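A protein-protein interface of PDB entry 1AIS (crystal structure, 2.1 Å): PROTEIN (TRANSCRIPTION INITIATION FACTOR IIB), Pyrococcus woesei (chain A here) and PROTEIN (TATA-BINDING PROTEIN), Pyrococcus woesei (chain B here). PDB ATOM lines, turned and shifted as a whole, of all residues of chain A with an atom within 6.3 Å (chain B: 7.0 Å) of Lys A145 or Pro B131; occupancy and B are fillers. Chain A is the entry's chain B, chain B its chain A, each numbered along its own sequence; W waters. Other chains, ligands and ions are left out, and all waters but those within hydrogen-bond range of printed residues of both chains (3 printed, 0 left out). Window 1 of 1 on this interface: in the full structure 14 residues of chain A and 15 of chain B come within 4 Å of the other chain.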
ATOM      1  N   LEU A 141       4.495  10.931 -26.046  1.00  0.00           N
ATOM      2  CA  LEU A 141       4.748  12.289 -25.533  1.00  0.00           C
ATOM      3  C   LEU A 141       6.213  12.489 -25.171  1.00  0.00           C
ATOM      4  O   LEU A 141       6.580  13.509 -24.581  1.00  0.00           O
ATOM      5  CB  LEU A 141       3.949  12.512 -24.244  1.00  0.00           C
ATOM      6  CG  LEU A 141       2.475  12.102 -24.200  1.00  0.00           C
ATOM      7  CD1 LEU A 141       1.955  12.176 -22.767  1.00  0.00           C
ATOM      8  CD2 LEU A 141       1.665  12.987 -25.127  1.00  0.00           C
ATOM      9  N   THR A 142       7.049  11.533 -25.549  1.00  0.00           N
ATOM     10  CA  THR A 142       8.443  11.550 -25.146  1.00  0.00           C
ATOM     11  C   THR A 142       9.496  11.768 -26.209  1.00  0.00           C
ATOM     12  O   THR A 142      10.604  12.199 -25.899  1.00  0.00           O
ATOM     13  CB  THR A 142       8.781  10.219 -24.445  1.00  0.00           C
ATOM     14  OG1 THR A 142       8.527   9.136 -25.360  1.00  0.00           O
ATOM     15  CG2 THR A 142       7.928  10.017 -23.167  1.00  0.00           C
ATOM     16  N   SER A 143       9.167  11.430 -27.451  1.00  0.00           N
ATOM     17  CA  SER A 143      10.108  11.551 -28.566  1.00  0.00           C
ATOM     18  C   SER A 143      10.770  12.927 -28.661  1.00  0.00           C
ATOM     19  O   SER A 143      10.082  13.950 -28.688  1.00  0.00           O
ATOM     20  CB  SER A 143       9.405  11.232 -29.893  1.00  0.00           C
ATOM     21  OG  SER A 143      10.345  11.133 -30.947  1.00  0.00           O
ATOM     22  N   GLY A 144      12.103  12.940 -28.686  1.00  0.00           N
ATOM     23  CA  GLY A 144      12.828  14.194 -28.802  1.00  0.00           C
ATOM     24  C   GLY A 144      13.197  14.864 -27.498  1.00  0.00           C
ATOM     25  O   GLY A 144      14.130  15.666 -27.486  1.00  0.00           O
ATOM     26  N   LYS A 145      12.430  14.604 -26.430  1.00  0.00           N
ATOM     27  CA  LYS A 145      12.706  15.175 -25.095  1.00  0.00           C
ATOM     28  C   LYS A 145      13.891  14.473 -24.453  1.00  0.00           C
ATOM     29  O   LYS A 145      14.152  13.305 -24.738  1.00  0.00           O
ATOM     30  CB  LYS A 145      11.504  15.028 -24.167  1.00  0.00           C
ATOM     31  CG  LYS A 145      10.489  16.105 -24.305  1.00  0.00           C
ATOM     32  CD  LYS A 145       9.738  15.999 -25.587  1.00  0.00           C
ATOM     33  CE  LYS A 145       8.816  17.191 -25.721  1.00  0.00           C
ATOM     34  NZ  LYS A 145       7.924  17.088 -26.890  1.00  0.00           N
ATOM     35  N   SER A 146      14.612  15.171 -23.583  1.00  0.00           N
ATOM     36  CA  SER A 146      15.758  14.545 -22.928  1.00  0.00           C
ATOM     37  C   SER A 146      15.253  13.662 -21.799  1.00  0.00           C
ATOM     38  O   SER A 146      14.252  13.975 -21.181  1.00  0.00           O
ATOM     39  CB  SER A 146      16.716  15.604 -22.378  1.00  0.00           C
ATOM     40  OG  SER A 146      16.178  16.162 -21.196  1.00  0.00           O
ATOM     41  N   PRO A 147      15.915  12.517 -21.553  1.00  0.00           N
ATOM     42  CA  PRO A 147      15.531  11.578 -20.489  1.00  0.00           C
ATOM     43  C   PRO A 147      15.438  12.242 -19.101  1.00  0.00           C
ATOM     44  O   PRO A 147      14.474  12.028 -18.368  1.00  0.00           O
ATOM     45  CB  PRO A 147      16.659  10.546 -20.526  1.00  0.00           C
ATOM     46  CG  PRO A 147      17.075  10.548 -21.959  1.00  0.00           C
ATOM     47  CD  PRO A 147      17.073  12.010 -22.314  1.00  0.00           C
ATOM     48  N   LEU A 150      12.251  14.397 -18.540  1.00  0.00           N
ATOM     49  CA  LEU A 150      11.057  13.578 -18.414  1.00  0.00           C
ATOM     50  C   LEU A 150      11.006  12.865 -17.075  1.00  0.00           C
ATOM     51  O   LEU A 150       9.949  12.801 -16.448  1.00  0.00           O
ATOM     52  CB  LEU A 150      11.007  12.549 -19.552  1.00  0.00           C
ATOM     53  CG  LEU A 150      10.720  13.106 -20.950  1.00  0.00           C
ATOM     54  CD1 LEU A 150      11.029  12.073 -22.015  1.00  0.00           C
ATOM     55  CD2 LEU A 150       9.262  13.542 -21.023  1.00  0.00           C
ATOM     56  N   ARG A 185       8.124  19.948 -18.761  1.00  0.00           N
ATOM     57  CA  ARG A 185       7.793  18.524 -18.866  1.00  0.00           C
ATOM     58  C   ARG A 185       6.630  18.137 -17.979  1.00  0.00           C
ATOM     59  O   ARG A 185       5.745  17.396 -18.385  1.00  0.00           O
ATOM     60  CB  ARG A 185       8.997  17.671 -18.483  1.00  0.00           C
ATOM     61  CG  ARG A 185      10.212  17.856 -19.370  1.00  0.00           C
ATOM     62  CD  ARG A 185      10.006  17.251 -20.746  1.00  0.00           C
ATOM     63  NE  ARG A 185      10.275  18.281 -21.728  1.00  0.00           N
ATOM     64  CZ  ARG A 185       9.334  18.935 -22.397  1.00  0.00           C
ATOM     65  NH1 ARG A 185       8.053  18.645 -22.219  1.00  0.00           N
ATOM     66  NH2 ARG A 185       9.674  19.968 -23.145  1.00  0.00           N
ATOM     67  N   GLU A 188       3.145  19.387 -19.244  1.00  0.00           N
ATOM     68  CA  GLU A 188       2.729  18.625 -20.412  1.00  0.00           C
ATOM     69  C   GLU A 188       2.214  17.261 -19.982  1.00  0.00           C
ATOM     70  O   GLU A 188       1.164  16.828 -20.424  1.00  0.00           O
ATOM     71  CB  GLU A 188       3.895  18.454 -21.381  1.00  0.00           C
ATOM     72  CG  GLU A 188       3.478  17.758 -22.653  1.00  0.00           C
ATOM     73  CD  GLU A 188       4.637  17.353 -23.540  1.00  0.00           C
ATOM     74  OE1 GLU A 188       5.446  16.481 -23.135  1.00  0.00           O
ATOM     75  OE2 GLU A 188       4.710  17.881 -24.669  1.00  0.00           O
ATOM     76  N   ASP B 118      12.426   7.175 -31.182  1.00  0.00           N
ATOM     77  CA  ASP B 118      12.972   6.036 -30.445  1.00  0.00           C
ATOM     78  C   ASP B 118      12.870   4.819 -31.349  1.00  0.00           C
ATOM     79  O   ASP B 118      13.811   4.039 -31.459  1.00  0.00           O
ATOM     80  CB  ASP B 118      12.206   5.801 -29.146  1.00  0.00           C
ATOM     81  CG  ASP B 118      12.371   6.934 -28.161  1.00  0.00           C
ATOM     82  OD1 ASP B 118      13.489   7.072 -27.627  1.00  0.00           O
ATOM     83  OD2 ASP B 118      11.391   7.691 -27.933  1.00  0.00           O
ATOM     84  N   TYR B 129      21.214   8.838 -32.693  1.00  0.00           N
ATOM     85  CA  TYR B 129      20.191   9.508 -31.913  1.00  0.00           C
ATOM     86  C   TYR B 129      20.664   9.520 -30.471  1.00  0.00           C
ATOM     87  O   TYR B 129      20.944   8.480 -29.867  1.00  0.00           O
ATOM     88  CB  TYR B 129      18.820   8.835 -32.073  1.00  0.00           C
ATOM     89  CG  TYR B 129      17.683   9.540 -31.350  1.00  0.00           C
ATOM     90  CD1 TYR B 129      17.531  10.931 -31.423  1.00  0.00           C
ATOM     91  CD2 TYR B 129      16.769   8.813 -30.574  1.00  0.00           C
ATOM     92  CE1 TYR B 129      16.502  11.580 -30.744  1.00  0.00           C
ATOM     93  CE2 TYR B 129      15.741   9.456 -29.889  1.00  0.00           C
ATOM     94  CZ  TYR B 129      15.614  10.842 -29.976  1.00  0.00           C
ATOM     95  OH  TYR B 129      14.629  11.485 -29.249  1.00  0.00           O
ATOM     96  N   GLU B 130      20.811  10.727 -29.955  1.00  0.00           N
ATOM     97  CA  GLU B 130      21.263  10.945 -28.613  1.00  0.00           C
ATOM     98  C   GLU B 130      20.485  12.146 -28.099  1.00  0.00           C
ATOM     99  O   GLU B 130      21.000  13.273 -28.100  1.00  0.00           O
ATOM    100  CB  GLU B 130      22.765  11.255 -28.628  1.00  0.00           C
ATOM    101  CG  GLU B 130      23.643  10.135 -29.216  1.00  0.00           C
ATOM    102  CD  GLU B 130      23.626   8.847 -28.378  1.00  0.00           C
ATOM    103  OE1 GLU B 130      23.553   8.937 -27.127  1.00  0.00           O
ATOM    104  OE2 GLU B 130      23.673   7.746 -28.975  1.00  0.00           O
ATOM    105  N   PRO B 131      19.229  11.918 -27.650  1.00  0.00           N
ATOM    106  CA  PRO B 131      18.300  12.922 -27.112  1.00  0.00           C
ATOM    107  C   PRO B 131      18.802  13.609 -25.837  1.00  0.00           C
ATOM    108  O   PRO B 131      18.214  14.578 -25.352  1.00  0.00           O
ATOM    109  CB  PRO B 131      17.026  12.113 -26.879  1.00  0.00           C
ATOM    110  CG  PRO B 131      17.525  10.756 -26.608  1.00  0.00           C
ATOM    111  CD  PRO B 131      18.618  10.577 -27.606  1.00  0.00           C
ATOM    112  N   GLU B 132      19.905  13.096 -25.298  1.00  0.00           N
ATOM    113  CA  GLU B 132      20.518  13.665 -24.107  1.00  0.00           C
ATOM    114  C   GLU B 132      21.413  14.828 -24.553  1.00  0.00           C
ATOM    115  O   GLU B 132      21.730  15.723 -23.779  1.00  0.00           O
ATOM    116  CB  GLU B 132      21.346  12.592 -23.412  1.00  0.00           C
ATOM    117  CG  GLU B 132      21.520  12.820 -21.946  1.00  0.00           C
ATOM    118  CD  GLU B 132      22.669  12.031 -21.360  1.00  0.00           C
ATOM    119  OE1 GLU B 132      22.794  10.818 -21.652  1.00  0.00           O
ATOM    120  OE2 GLU B 132      23.452  12.641 -20.603  1.00  0.00           O
ATOM    121  N   GLN B 133      21.761  14.817 -25.836  1.00  0.00           N
ATOM    122  CA  GLN B 133      22.616  15.818 -26.450  1.00  0.00           C
ATOM    123  C   GLN B 133      21.917  16.662 -27.551  1.00  0.00           C
ATOM    124  O   GLN B 133      22.149  17.861 -27.647  1.00  0.00           O
ATOM    125  CB  GLN B 133      23.848  15.100 -27.020  1.00  0.00           C
ATOM    126  CG  GLN B 133      24.796  15.960 -27.833  1.00  0.00           C
ATOM    127  CD  GLN B 133      25.593  16.952 -26.991  1.00  0.00           C
ATOM    128  OE1 GLN B 133      26.798  16.775 -26.783  1.00  0.00           O
ATOM    129  NE2 GLN B 133      24.929  18.014 -26.524  1.00  0.00           N
ATOM    130  N   PHE B 134      21.036  16.047 -28.340  1.00  0.00           N
ATOM    131  CA  PHE B 134      20.348  16.745 -29.436  1.00  0.00           C
ATOM    132  C   PHE B 134      19.025  16.021 -29.744  1.00  0.00           C
ATOM    133  O   PHE B 134      18.967  14.788 -29.742  1.00  0.00           O
ATOM    134  CB  PHE B 134      21.269  16.769 -30.673  1.00  0.00           C
ATOM    135  CG  PHE B 134      20.754  17.601 -31.819  1.00  0.00           C
ATOM    136  CD1 PHE B 134      20.741  18.989 -31.737  1.00  0.00           C
ATOM    137  CD2 PHE B 134      20.282  16.993 -32.977  1.00  0.00           C
ATOM    138  CE1 PHE B 134      20.260  19.765 -32.784  1.00  0.00           C
ATOM    139  CE2 PHE B 134      19.799  17.750 -34.027  1.00  0.00           C
ATOM    140  CZ  PHE B 134      19.788  19.149 -33.931  1.00  0.00           C
ATOM    141  N   PRO B 135      17.949  16.775 -30.042  1.00  0.00           N
ATOM    142  CA  PRO B 135      16.647  16.166 -30.337  1.00  0.00           C
ATOM    143  C   PRO B 135      16.373  15.529 -31.707  1.00  0.00           C
ATOM    144  O   PRO B 135      15.255  15.051 -31.958  1.00  0.00           O
ATOM    145  CB  PRO B 135      15.676  17.309 -30.036  1.00  0.00           C
ATOM    146  CG  PRO B 135      16.440  18.502 -30.393  1.00  0.00           C
ATOM    147  CD  PRO B 135      17.811  18.229 -29.863  1.00  0.00           C
ATOM    148  N   GLY B 136      17.367  15.475 -32.585  1.00  0.00           N
ATOM    149  CA  GLY B 136      17.107  14.882 -33.888  1.00  0.00           C
ATOM    150  C   GLY B 136      17.942  13.668 -34.234  1.00  0.00           C
ATOM    151  O   GLY B 136      19.003  13.435 -33.650  1.00  0.00           O
ATOM    152  N   SER B 152      11.035  14.645 -34.583  1.00  0.00           N
ATOM    153  CA  SER B 152       9.751  14.008 -34.281  1.00  0.00           C
ATOM    154  C   SER B 152       8.583  14.638 -34.994  1.00  0.00           C
ATOM    155  O   SER B 152       7.612  13.965 -35.354  1.00  0.00           O
ATOM    156  CB  SER B 152       9.498  14.039 -32.774  1.00  0.00           C
ATOM    157  OG  SER B 152      10.593  13.445 -32.105  1.00  0.00           O
HETATM  158  O   HOH W   1      16.750  16.172 -26.789  1.00  0.00           O
HETATM  159  O   HOH W   2      13.285   9.977 -27.402  1.00  0.00           O
HETATM  160  O   HOH W   3      10.721  16.174 -30.454  1.00  0.00           O
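Water W1 lies within hydrogen-bond range of the backbone carbonyl oxygen of Pro B131 and the backbone carbonyl oxygen of Gly A144. Water W2 lies within hydrogen-bond range of the side-chain hydroxyl of Tyr B129 (2.7 Å), the side-chain carboxylate of Asp B118 (2.9 Å) and the backbone NH of Gly A144 (3.4 Å). Water W3 bridges the backbone carbonyl oxygen (O) of Ser A143 (2.9 Å) and the side-chain hydroxyl (OG) of Ser B152 (3.2 Å).
The side-chain hydroxyl (OG) of Ser A143 lies within hydrogen-bond range of the side-chain hydroxyl (OG) of Ser B152. The side-chain hydroxyl of Tyr B129 is in hydrogen-bond range of the backbone NH of Gly A144, 3.0 Å away.
NZ of Lys A145 lies within salt-bridge range of OE2 of Glu A188.
Of the printed residues of chain B, Ser A143 touches Ser B152 (2.6 Å). Of the printed residues of chain B, Gly A144 touches Tyr B129 (3.0 Å), Pro B135 (3.4 Å) and Ser B152 (3.8 Å). Lys A145 touches just one residue of chain B: Pro B131. Printed residues of chain B within 4 Å of Ser A146: Pro B131 (3.5 Å). Pro B131 touches just these residues of chain A: Lys A145 (3.8 Å) and Ser A146 (3.5 Å). Printed residues of chain A within 4 Å of Ser B152: Ser A143 (2.6 Å) and Gly A144 (3.8 Å).
Among the printed residues, merely in contact across the chains: Gly A144 with Pro B135 (3.4 Å), Gly A144 with Ser B152 (3.8 Å), Lys A145 with Pro B131 (3.8 Å) and Ser A146 with Pro B131 (3.5 Å).
Hydrophobic or aromatic side chains of chain B within 4 Å of the printed part of chain A: Tyr B129, Pro B131 and Pro B135. Along chain A the printed residues that touch a printed residue of chain B span positions 143 to 146. Among the printed residues, no Asp or Glu carboxylate lies within 4 Å of a Lys or Arg side-chain nitrogen of the other chain.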
